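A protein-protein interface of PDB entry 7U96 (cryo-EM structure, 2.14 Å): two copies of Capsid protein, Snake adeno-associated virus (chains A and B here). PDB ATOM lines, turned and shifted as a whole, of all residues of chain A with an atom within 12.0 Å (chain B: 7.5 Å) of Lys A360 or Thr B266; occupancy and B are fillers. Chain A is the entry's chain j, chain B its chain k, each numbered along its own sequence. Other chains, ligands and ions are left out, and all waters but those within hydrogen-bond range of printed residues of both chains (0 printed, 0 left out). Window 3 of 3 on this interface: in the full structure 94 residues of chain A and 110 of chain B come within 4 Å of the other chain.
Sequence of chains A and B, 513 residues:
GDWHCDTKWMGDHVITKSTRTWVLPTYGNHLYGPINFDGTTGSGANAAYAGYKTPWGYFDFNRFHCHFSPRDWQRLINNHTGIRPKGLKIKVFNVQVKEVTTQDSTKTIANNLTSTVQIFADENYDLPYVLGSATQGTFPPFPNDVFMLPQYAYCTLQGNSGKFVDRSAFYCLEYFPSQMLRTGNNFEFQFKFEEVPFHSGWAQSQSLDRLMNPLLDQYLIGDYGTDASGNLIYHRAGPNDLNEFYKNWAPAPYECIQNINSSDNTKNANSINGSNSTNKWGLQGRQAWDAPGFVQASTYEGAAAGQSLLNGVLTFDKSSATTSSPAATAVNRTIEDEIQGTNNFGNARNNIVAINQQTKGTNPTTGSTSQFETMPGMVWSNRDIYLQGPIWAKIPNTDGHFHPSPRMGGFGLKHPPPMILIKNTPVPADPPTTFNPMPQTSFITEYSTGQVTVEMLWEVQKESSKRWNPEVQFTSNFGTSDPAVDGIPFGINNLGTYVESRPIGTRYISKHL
Hydrophobic or aromatic side chains of chain B within 4 Å of the printed part of chain A: Ala B269.
Of the 18 printed residues of chain A, 10 touch a printed residue of chain B.
Printed residues of chain A that touch a printed residue of chain B: Thr A226, Asp A227, Ala A228, Ser A229, Gly A230, Asn A231, Gln A358, Thr A359, Lys A360 and Thr A362.
Among the printed residues, 23 pairs touch across the chains.
Among the printed residues, pairs that only touch across the chains: Lys A360 with Thr B266, Gly A230 with Asn B265, Thr A359 with Ala B269, Thr A359 with Lys B267, Ser A229 with Asn B270, Gly A230 with Asn B270, Ser A229 with Asn B265, Thr A362 with Ala B269, Lys A360 with Ala B269, Ala A228 with Ser B271, Thr A226 with Asn B270, Gln A358 with Asn B268 and Asp A227 with Asn B270.
The side-chain carboxylate (OD1) of Asp B264 lies within hydrogen-bond range of the side-chain hydroxyl (OG1) of Thr B266, 2.8 Å away.
The side-chain carboxylate (OD1) of Asp A227 is in hydrogen-bond range of the backbone NH (N) of Gly A230 (2.9 Å).
The backbone NH (N) of Asn A231 sits at hydrogen-bond distance from the side-chain carboxylate (OD1) of Asp A227 (2.5 Å).
OD1 of Asn B268 lies close to O of Asn B261 (2.8 Å).
The side-chain carboxylate (OD2) of Asp B264 is in salt-bridge range of the side-chain amino group (NZ) of Lys B267 (3.3 Å).
OD1 of Asp A227 lies close to N of Ser A229 (3.3 Å).
No position is printed for both chains.
The backbone carbonyl oxygen (O) of Lys B267 is in hydrogen-bond range of the backbone NH (N) of Lys A360 (3.2 Å).
The side-chain amide nitrogen (ND2) of Asn A231 lies close to the side-chain amide nitrogen (ND2) of Asn B265, 3.2 Å away.
The side-chain amino group of Lys A360 lies within hydrogen-bond range of the backbone carbonyl oxygen of Asn B265, at 3.5 Å.
OD1 of Asn B268 sits close to O of Gly A230.
NZ of Lys A360 is in hydrogen-bond range of O of Asn B268 (2.9 Å).
O of Asp A227 is in hydrogen-bond range of N of Ser B271.
The backbone carbonyl oxygen (O) of Ala A228 lies close to the side-chain amide oxygen (OD1) of Asn B270, at 3.2 Å.
NZ of Lys A360 is in hydrogen-bond range of OD1 of Asn B270 (3.0 Å).
The side-chain hydroxyl (OG1) of Thr A226 sits at hydrogen-bond distance from the backbone NH (N) of Ser B271, 3.3 Å away.
OG1 of Thr A226 is in hydrogen-bond range of O of Ala B269 (3.0 Å).
Of the printed residues of chain B, Thr A226 touches Ala B269, Asn B270 and Ser B271.
Printed residues of chain B within 4 Å of Asp A227: Asn B270 (3.95 Å) and Ser B271 (3.0 Å).
Printed residues of chain B within 4 Å of Asn A231: Asn B265.
Of chain B, only Asn B265, Thr B266, Lys B267, Asn B268, Ala B269 and Asn B270 come within 4 Å of Lys A360.
Printed residues of chain B within 4 Å of Thr A362: Ala B269.
Thr A365 touches none of the printed residues of chain B.
No residue of chain A comes within 4 Å of Asp B264.
Thr B266 touches just one residue of chain A: Lys A360.
Lys B267 touches just these residues of chain A: Thr A359 (3.4 Å) and Lys A360 (3.2 Å).
Of chain A, only Gly A230, Gln A358 and Lys A360 come within 4 Å of Asn B268.
Ala B269 touches four residues of chain A.
Of the printed residues of chain A, Asn B270 touches Thr A226 (3.8 Å), Asp A227 (3.95 Å), Ala A228 (3.1 Å), Ser A229 (3.5 Å), Gly A230 (3.6 Å) and Lys A360 (3.0 Å).
Of the printed residues of chain A, Ser B271 touches Thr A226, Asp A227 and Ala A228.
The nearest residue of chain B that does not touch Lys A360 is Asp B264 (7.2 Å).
The nearest residue of chain A that does not touch Thr B266 is Ser A229 (5.5 Å).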
ATOM      1  N   GLY A 225     -17.586  -4.784  -5.242  1.00  0.00           N
ATOM      2  CA  GLY A 225     -18.129  -3.444  -5.309  1.00  0.00           C
ATOM      3  C   GLY A 225     -18.063  -2.895  -6.719  1.00  0.00           C
ATOM      4  O   GLY A 225     -17.984  -3.644  -7.697  1.00  0.00           O
ATOM      5  N   THR A 226     -18.108  -1.569  -6.829  1.00  0.00           N
ATOM      6  CA  THR A 226     -17.834  -0.883  -8.083  1.00  0.00           C
ATOM      7  C   THR A 226     -16.731   0.141  -7.871  1.00  0.00           C
ATOM      8  O   THR A 226     -16.471   0.582  -6.751  1.00  0.00           O
ATOM      9  CB  THR A 226     -19.069  -0.178  -8.672  1.00  0.00           C
ATOM     10  OG1 THR A 226     -19.579   0.779  -7.739  1.00  0.00           O
ATOM     11  CG2 THR A 226     -20.148  -1.175  -9.027  1.00  0.00           C
ATOM     12  N   ASP A 227     -16.088   0.519  -8.968  1.00  0.00           N
ATOM     13  CA  ASP A 227     -15.044   1.532  -8.933  1.00  0.00           C
ATOM     14  C   ASP A 227     -15.673   2.908  -9.137  1.00  0.00           C
ATOM     15  O   ASP A 227     -16.896   3.065  -9.118  1.00  0.00           O
ATOM     16  CB  ASP A 227     -13.961   1.215  -9.961  1.00  0.00           C
ATOM     17  CG  ASP A 227     -14.478   1.221 -11.384  1.00  0.00           C
ATOM     18  OD1 ASP A 227     -15.692   1.380 -11.597  1.00  0.00           O
ATOM     19  OD2 ASP A 227     -13.656   1.057 -12.303  1.00  0.00           O
ATOM     20  N   ALA A 228     -14.839   3.928  -9.337  1.00  0.00           N
ATOM     21  CA  ALA A 228     -15.350   5.291  -9.437  1.00  0.00           C
ATOM     22  C   ALA A 228     -16.155   5.494 -10.711  1.00  0.00           C
ATOM     23  O   ALA A 228     -16.999   6.391 -10.785  1.00  0.00           O
ATOM     24  CB  ALA A 228     -14.196   6.289  -9.368  1.00  0.00           C
ATOM     25  N   SER A 229     -15.908   4.675 -11.728  1.00  0.00           N
ATOM     26  CA  SER A 229     -16.671   4.759 -12.963  1.00  0.00           C
ATOM     27  C   SER A 229     -17.890   3.847 -12.973  1.00  0.00           C
ATOM     28  O   SER A 229     -18.699   3.934 -13.900  1.00  0.00           O
ATOM     29  CB  SER A 229     -15.769   4.424 -14.148  1.00  0.00           C
ATOM     30  OG  SER A 229     -16.497   4.447 -15.358  1.00  0.00           O
ATOM     31  N   GLY A 230     -18.047   2.984 -11.977  1.00  0.00           N
ATOM     32  CA  GLY A 230     -19.162   2.067 -11.945  1.00  0.00           C
ATOM     33  C   GLY A 230     -18.896   0.694 -12.517  1.00  0.00           C
ATOM     34  O   GLY A 230     -19.850  -0.003 -12.868  1.00  0.00           O
ATOM     35  N   ASN A 231     -17.639   0.287 -12.635  1.00  0.00           N
ATOM     36  CA  ASN A 231     -17.322  -1.052 -13.105  1.00  0.00           C
ATOM     37  C   ASN A 231     -17.253  -2.025 -11.939  1.00  0.00           C
ATOM     38  O   ASN A 231     -16.701  -1.716 -10.883  1.00  0.00           O
ATOM     39  CB  ASN A 231     -15.996  -1.051 -13.859  1.00  0.00           C
ATOM     40  CG  ASN A 231     -16.056  -0.253 -15.136  1.00  0.00           C
ATOM     41  OD1 ASN A 231     -15.263   0.657 -15.346  1.00  0.00           O
ATOM     42  ND2 ASN A 231     -16.976  -0.613 -16.016  1.00  0.00           N
ATOM     43  N   LEU A 232     -17.813  -3.209 -12.146  1.00  0.00           N
ATOM     44  CA  LEU A 232     -17.814  -4.246 -11.127  1.00  0.00           C
ATOM     45  C   LEU A 232     -16.393  -4.710 -10.819  1.00  0.00           C
ATOM     46  O   LEU A 232     -15.583  -4.919 -11.721  1.00  0.00           O
ATOM     47  CB  LEU A 232     -18.677  -5.413 -11.605  1.00  0.00           C
ATOM     48  CG  LEU A 232     -18.850  -6.675 -10.769  1.00  0.00           C
ATOM     49  CD1 LEU A 232     -19.556  -6.371  -9.464  1.00  0.00           C
ATOM     50  CD2 LEU A 232     -19.614  -7.712 -11.567  1.00  0.00           C
ATOM     51  N   ASN A 356     -33.500  -1.237  -1.032  1.00  0.00           N
ATOM     52  CA  ASN A 356     -33.881  -0.416  -2.181  1.00  0.00           C
ATOM     53  C   ASN A 356     -33.316  -1.005  -3.467  1.00  0.00           C
ATOM     54  O   ASN A 356     -32.739  -2.091  -3.478  1.00  0.00           O
ATOM     55  CB  ASN A 356     -33.445   1.049  -2.019  1.00  0.00           C
ATOM     56  CG  ASN A 356     -31.945   1.248  -2.138  1.00  0.00           C
ATOM     57  OD1 ASN A 356     -31.165   0.307  -2.087  1.00  0.00           O
ATOM     58  ND2 ASN A 356     -31.541   2.493  -2.307  1.00  0.00           N
ATOM     59  N   GLN A 357     -33.502  -0.263  -4.554  1.00  0.00           N
ATOM     60  CA  GLN A 357     -33.017  -0.628  -5.880  1.00  0.00           C
ATOM     61  C   GLN A 357     -32.041   0.441  -6.346  1.00  0.00           C
ATOM     62  O   GLN A 357     -32.426   1.599  -6.528  1.00  0.00           O
ATOM     63  CB  GLN A 357     -34.173  -0.755  -6.869  1.00  0.00           C
ATOM     64  CG  GLN A 357     -35.151  -1.857  -6.544  1.00  0.00           C
ATOM     65  CD  GLN A 357     -36.322  -1.887  -7.492  1.00  0.00           C
ATOM     66  OE1 GLN A 357     -36.685  -0.872  -8.077  1.00  0.00           O
ATOM     67  NE2 GLN A 357     -36.917  -3.055  -7.659  1.00  0.00           N
ATOM     68  N   GLN A 358     -30.788   0.055  -6.551  1.00  0.00           N
ATOM     69  CA  GLN A 358     -29.733   1.012  -6.840  1.00  0.00           C
ATOM     70  C   GLN A 358     -29.631   1.287  -8.336  1.00  0.00           C
ATOM     71  O   GLN A 358     -29.837   0.396  -9.166  1.00  0.00           O
ATOM     72  CB  GLN A 358     -28.393   0.496  -6.337  1.00  0.00           C
ATOM     73  CG  GLN A 358     -27.935  -0.645  -7.173  1.00  0.00           C
ATOM     74  CD  GLN A 358     -26.593  -1.134  -6.825  1.00  0.00           C
ATOM     75  OE1 GLN A 358     -26.134  -0.983  -5.695  1.00  0.00           O
ATOM     76  NE2 GLN A 358     -25.917  -1.707  -7.806  1.00  0.00           N
ATOM     77  N   THR A 359     -29.354   2.541  -8.672  1.00  0.00           N
ATOM     78  CA  THR A 359     -28.996   2.967 -10.019  1.00  0.00           C
ATOM     79  C   THR A 359     -27.943   4.050  -9.880  1.00  0.00           C
ATOM     80  O   THR A 359     -27.641   4.502  -8.776  1.00  0.00           O
ATOM     81  CB  THR A 359     -30.191   3.497 -10.830  1.00  0.00           C
ATOM     82  OG1 THR A 359     -30.780   4.617 -10.160  1.00  0.00           O
ATOM     83  CG2 THR A 359     -31.243   2.433 -11.043  1.00  0.00           C
ATOM     84  N   LYS A 360     -27.364   4.455 -11.004  1.00  0.00           N
ATOM     85  CA  LYS A 360     -26.474   5.606 -10.975  1.00  0.00           C
ATOM     86  C   LYS A 360     -27.227   6.827 -10.469  1.00  0.00           C
ATOM     87  O   LYS A 360     -28.270   7.199 -11.012  1.00  0.00           O
ATOM     88  CB  LYS A 360     -25.887   5.873 -12.355  1.00  0.00           C
ATOM     89  CG  LYS A 360     -24.825   6.953 -12.341  1.00  0.00           C
ATOM     90  CD  LYS A 360     -24.154   7.081 -13.677  1.00  0.00           C
ATOM     91  CE  LYS A 360     -23.378   5.815 -14.011  1.00  0.00           C
ATOM     92  NZ  LYS A 360     -22.268   5.546 -13.069  1.00  0.00           N
ATOM     93  N   GLY A 361     -26.695   7.444  -9.421  1.00  0.00           N
ATOM     94  CA  GLY A 361     -27.363   8.527  -8.740  1.00  0.00           C
ATOM     95  C   GLY A 361     -28.013   8.168  -7.418  1.00  0.00           C
ATOM     96  O   GLY A 361     -28.247   9.068  -6.604  1.00  0.00           O
ATOM     97  N   THR A 362     -28.314   6.894  -7.168  1.00  0.00           N
ATOM     98  CA  THR A 362     -28.903   6.469  -5.902  1.00  0.00           C
ATOM     99  C   THR A 362     -28.098   5.312  -5.329  1.00  0.00           C
ATOM    100  O   THR A 362     -27.887   4.299  -6.001  1.00  0.00           O
ATOM    101  CB  THR A 362     -30.388   6.102  -6.068  1.00  0.00           C
ATOM    102  OG1 THR A 362     -30.934   5.679  -4.813  1.00  0.00           O
ATOM    103  CG2 THR A 362     -30.600   5.036  -7.108  1.00  0.00           C
ATOM    104  N   ASN A 363     -27.642   5.470  -4.101  1.00  0.00           N
ATOM    105  CA  ASN A 363     -26.714   4.526  -3.500  1.00  0.00           C
ATOM    106  C   ASN A 363     -27.468   3.367  -2.855  1.00  0.00           C
ATOM    107  O   ASN A 363     -28.574   3.550  -2.346  1.00  0.00           O
ATOM    108  CB  ASN A 363     -25.857   5.224  -2.456  1.00  0.00           C
ATOM    109  CG  ASN A 363     -24.924   6.243  -3.059  1.00  0.00           C
ATOM    110  OD1 ASN A 363     -24.590   6.174  -4.237  1.00  0.00           O
ATOM    111  ND2 ASN A 363     -24.497   7.201  -2.253  1.00  0.00           N
ATOM    112  N   PRO A 364     -26.894   2.168  -2.860  1.00  0.00           N
ATOM    113  CA  PRO A 364     -27.566   1.029  -2.229  1.00  0.00           C
ATOM    114  C   PRO A 364     -27.647   1.189  -0.720  1.00  0.00           C
ATOM    115  O   PRO A 364     -26.717   1.683  -0.080  1.00  0.00           O
ATOM    116  CB  PRO A 364     -26.686  -0.159  -2.622  1.00  0.00           C
ATOM    117  CG  PRO A 364     -25.357   0.437  -2.872  1.00  0.00           C
ATOM    118  CD  PRO A 364     -25.608   1.785  -3.460  1.00  0.00           C
ATOM    119  N   THR A 365     -28.777   0.774  -0.156  1.00  0.00           N
ATOM    120  CA  THR A 365     -29.015   0.861   1.276  1.00  0.00           C
ATOM    121  C   THR A 365     -29.478  -0.486   1.809  1.00  0.00           C
ATOM    122  O   THR A 365     -30.092  -1.279   1.095  1.00  0.00           O
ATOM    123  CB  THR A 365     -30.055   1.932   1.618  1.00  0.00           C
ATOM    124  OG1 THR A 365     -31.289   1.630   0.963  1.00  0.00           O
ATOM    125  CG2 THR A 365     -29.581   3.300   1.174  1.00  0.00           C
ATOM    126  N   ASN B 261     -25.155  -4.537 -12.319  1.00  0.00           N
ATOM    127  CA  ASN B 261     -25.049  -4.747 -13.757  1.00  0.00           C
ATOM    128  C   ASN B 261     -23.599  -5.042 -14.107  1.00  0.00           C
ATOM    129  O   ASN B 261     -22.714  -4.223 -13.853  1.00  0.00           O
ATOM    130  CB  ASN B 261     -25.574  -3.541 -14.533  1.00  0.00           C
ATOM    131  CG  ASN B 261     -25.717  -3.816 -16.017  1.00  0.00           C
ATOM    132  OD1 ASN B 261     -24.977  -4.598 -16.599  1.00  0.00           O
ATOM    133  ND2 ASN B 261     -26.723  -3.217 -16.620  1.00  0.00           N
ATOM    134  N   SER B 263     -22.311  -5.893 -17.319  1.00  0.00           N
ATOM    135  CA  SER B 263     -21.854  -5.377 -18.605  1.00  0.00           C
ATOM    136  C   SER B 263     -21.713  -3.861 -18.654  1.00  0.00           C
ATOM    137  O   SER B 263     -20.680  -3.353 -19.091  1.00  0.00           O
ATOM    138  CB  SER B 263     -22.801  -5.831 -19.719  1.00  0.00           C
ATOM    139  OG  SER B 263     -22.763  -7.233 -19.871  1.00  0.00           O
ATOM    140  N   ASP B 264     -22.728  -3.127 -18.211  1.00  0.00           N
ATOM    141  CA  ASP B 264     -22.891  -1.710 -18.523  1.00  0.00           C
ATOM    142  C   ASP B 264     -22.716  -0.883 -17.258  1.00  0.00           C
ATOM    143  O   ASP B 264     -23.519  -0.992 -16.328  1.00  0.00           O
ATOM    144  CB  ASP B 264     -24.266  -1.463 -19.141  1.00  0.00           C
ATOM    145  CG  ASP B 264     -24.467  -0.028 -19.583  1.00  0.00           C
ATOM    146  OD1 ASP B 264     -23.520   0.780 -19.496  1.00  0.00           O
ATOM    147  OD2 ASP B 264     -25.588   0.294 -20.022  1.00  0.00           O
ATOM    148  N   ASN B 265     -21.688  -0.033 -17.240  1.00  0.00           N
ATOM    149  CA  ASN B 265     -21.376   0.700 -16.018  1.00  0.00           C
ATOM    150  C   ASN B 265     -22.268   1.919 -15.830  1.00  0.00           C
ATOM    151  O   ASN B 265     -22.280   2.504 -14.744  1.00  0.00           O
ATOM    152  CB  ASN B 265     -19.897   1.099 -15.998  1.00  0.00           C
ATOM    153  CG  ASN B 265     -19.506   2.014 -17.143  1.00  0.00           C
ATOM    154  OD1 ASN B 265     -20.284   2.845 -17.599  1.00  0.00           O
ATOM    155  ND2 ASN B 265     -18.281   1.864 -17.610  1.00  0.00           N
ATOM    156  N   THR B 266     -23.020   2.318 -16.856  1.00  0.00           N
ATOM    157  CA  THR B 266     -23.898   3.473 -16.700  1.00  0.00           C
ATOM    158  C   THR B 266     -25.081   3.145 -15.801  1.00  0.00           C
ATOM    159  O   THR B 266     -25.734   4.046 -15.268  1.00  0.00           O
ATOM    160  CB  THR B 266     -24.388   3.964 -18.061  1.00  0.00           C
ATOM    161  OG1 THR B 266     -25.108   2.919 -18.721  1.00  0.00           O
ATOM    162  CG2 THR B 266     -23.220   4.390 -18.927  1.00  0.00           C
ATOM    163  N   LYS B 267     -25.379   1.858 -15.629  1.00  0.00           N
ATOM    164  CA  LYS B 267     -26.497   1.466 -14.780  1.00  0.00           C
ATOM    165  C   LYS B 267     -26.109   1.438 -13.307  1.00  0.00           C
ATOM    166  O   LYS B 267     -26.969   1.574 -12.433  1.00  0.00           O
ATOM    167  CB  LYS B 267     -27.032   0.109 -15.221  1.00  0.00           C
ATOM    168  CG  LYS B 267     -27.531   0.085 -16.645  1.00  0.00           C
ATOM    169  CD  LYS B 267     -28.777   0.925 -16.785  1.00  0.00           C
ATOM    170  CE  LYS B 267     -29.357   0.825 -18.179  1.00  0.00           C
ATOM    171  NZ  LYS B 267     -28.490   1.496 -19.179  1.00  0.00           N
ATOM    172  N   ASN B 268     -24.836   1.217 -13.006  1.00  0.00           N
ATOM    173  CA  ASN B 268     -24.413   1.114 -11.618  1.00  0.00           C
ATOM    174  C   ASN B 268     -24.151   2.480 -10.999  1.00  0.00           C
ATOM    175  O   ASN B 268     -23.800   3.443 -11.680  1.00  0.00           O
ATOM    176  CB  ASN B 268     -23.163   0.250 -11.500  1.00  0.00           C
ATOM    177  CG  ASN B 268     -23.400  -1.164 -11.944  1.00  0.00           C
ATOM    178  OD1 ASN B 268     -22.621  -1.722 -12.704  1.00  0.00           O
ATOM    179  ND2 ASN B 268     -24.491  -1.750 -11.489  1.00  0.00           N
ATOM    180  N   ALA B 269     -24.316   2.547  -9.685  1.00  0.00           N
ATOM    181  CA  ALA B 269     -23.858   3.687  -8.909  1.00  0.00           C
ATOM    182  C   ALA B 269     -22.344   3.642  -8.745  1.00  0.00           C
ATOM    183  O   ALA B 269     -21.716   2.590  -8.875  1.00  0.00           O
ATOM    184  CB  ALA B 269     -24.527   3.708  -7.538  1.00  0.00           C
ATOM    185  N   ASN B 270     -21.761   4.795  -8.444  1.00  0.00           N
ATOM    186  CA  ASN B 270     -20.314   4.891  -8.331  1.00  0.00           C
ATOM    187  C   ASN B 270     -19.849   4.531  -6.926  1.00  0.00           C
ATOM    188  O   ASN B 270     -20.477   4.901  -5.932  1.00  0.00           O
ATOM    189  CB  ASN B 270     -19.853   6.302  -8.682  1.00  0.00           C
ATOM    190  CG  ASN B 270     -20.062   6.634 -10.139  1.00  0.00           C
ATOM    191  OD1 ASN B 270     -20.114   5.749 -10.984  1.00  0.00           O
ATOM    192  ND2 ASN B 270     -20.200   7.917 -10.438  1.00  0.00           N
ATOM    193  N   SER B 271     -18.740   3.794  -6.854  1.00  0.00           N
ATOM    194  CA  SER B 271     -18.036   3.521  -5.597  1.00  0.00           C
ATOM    195  C   SER B 271     -18.897   2.744  -4.604  1.00  0.00           C
ATOM    196  O   SER B 271     -18.952   3.069  -3.418  1.00  0.00           O
ATOM    197  CB  SER B 271     -17.522   4.814  -4.966  1.00  0.00           C
ATOM    198  OG  SER B 271     -16.541   5.416  -5.786  1.00  0.00           O
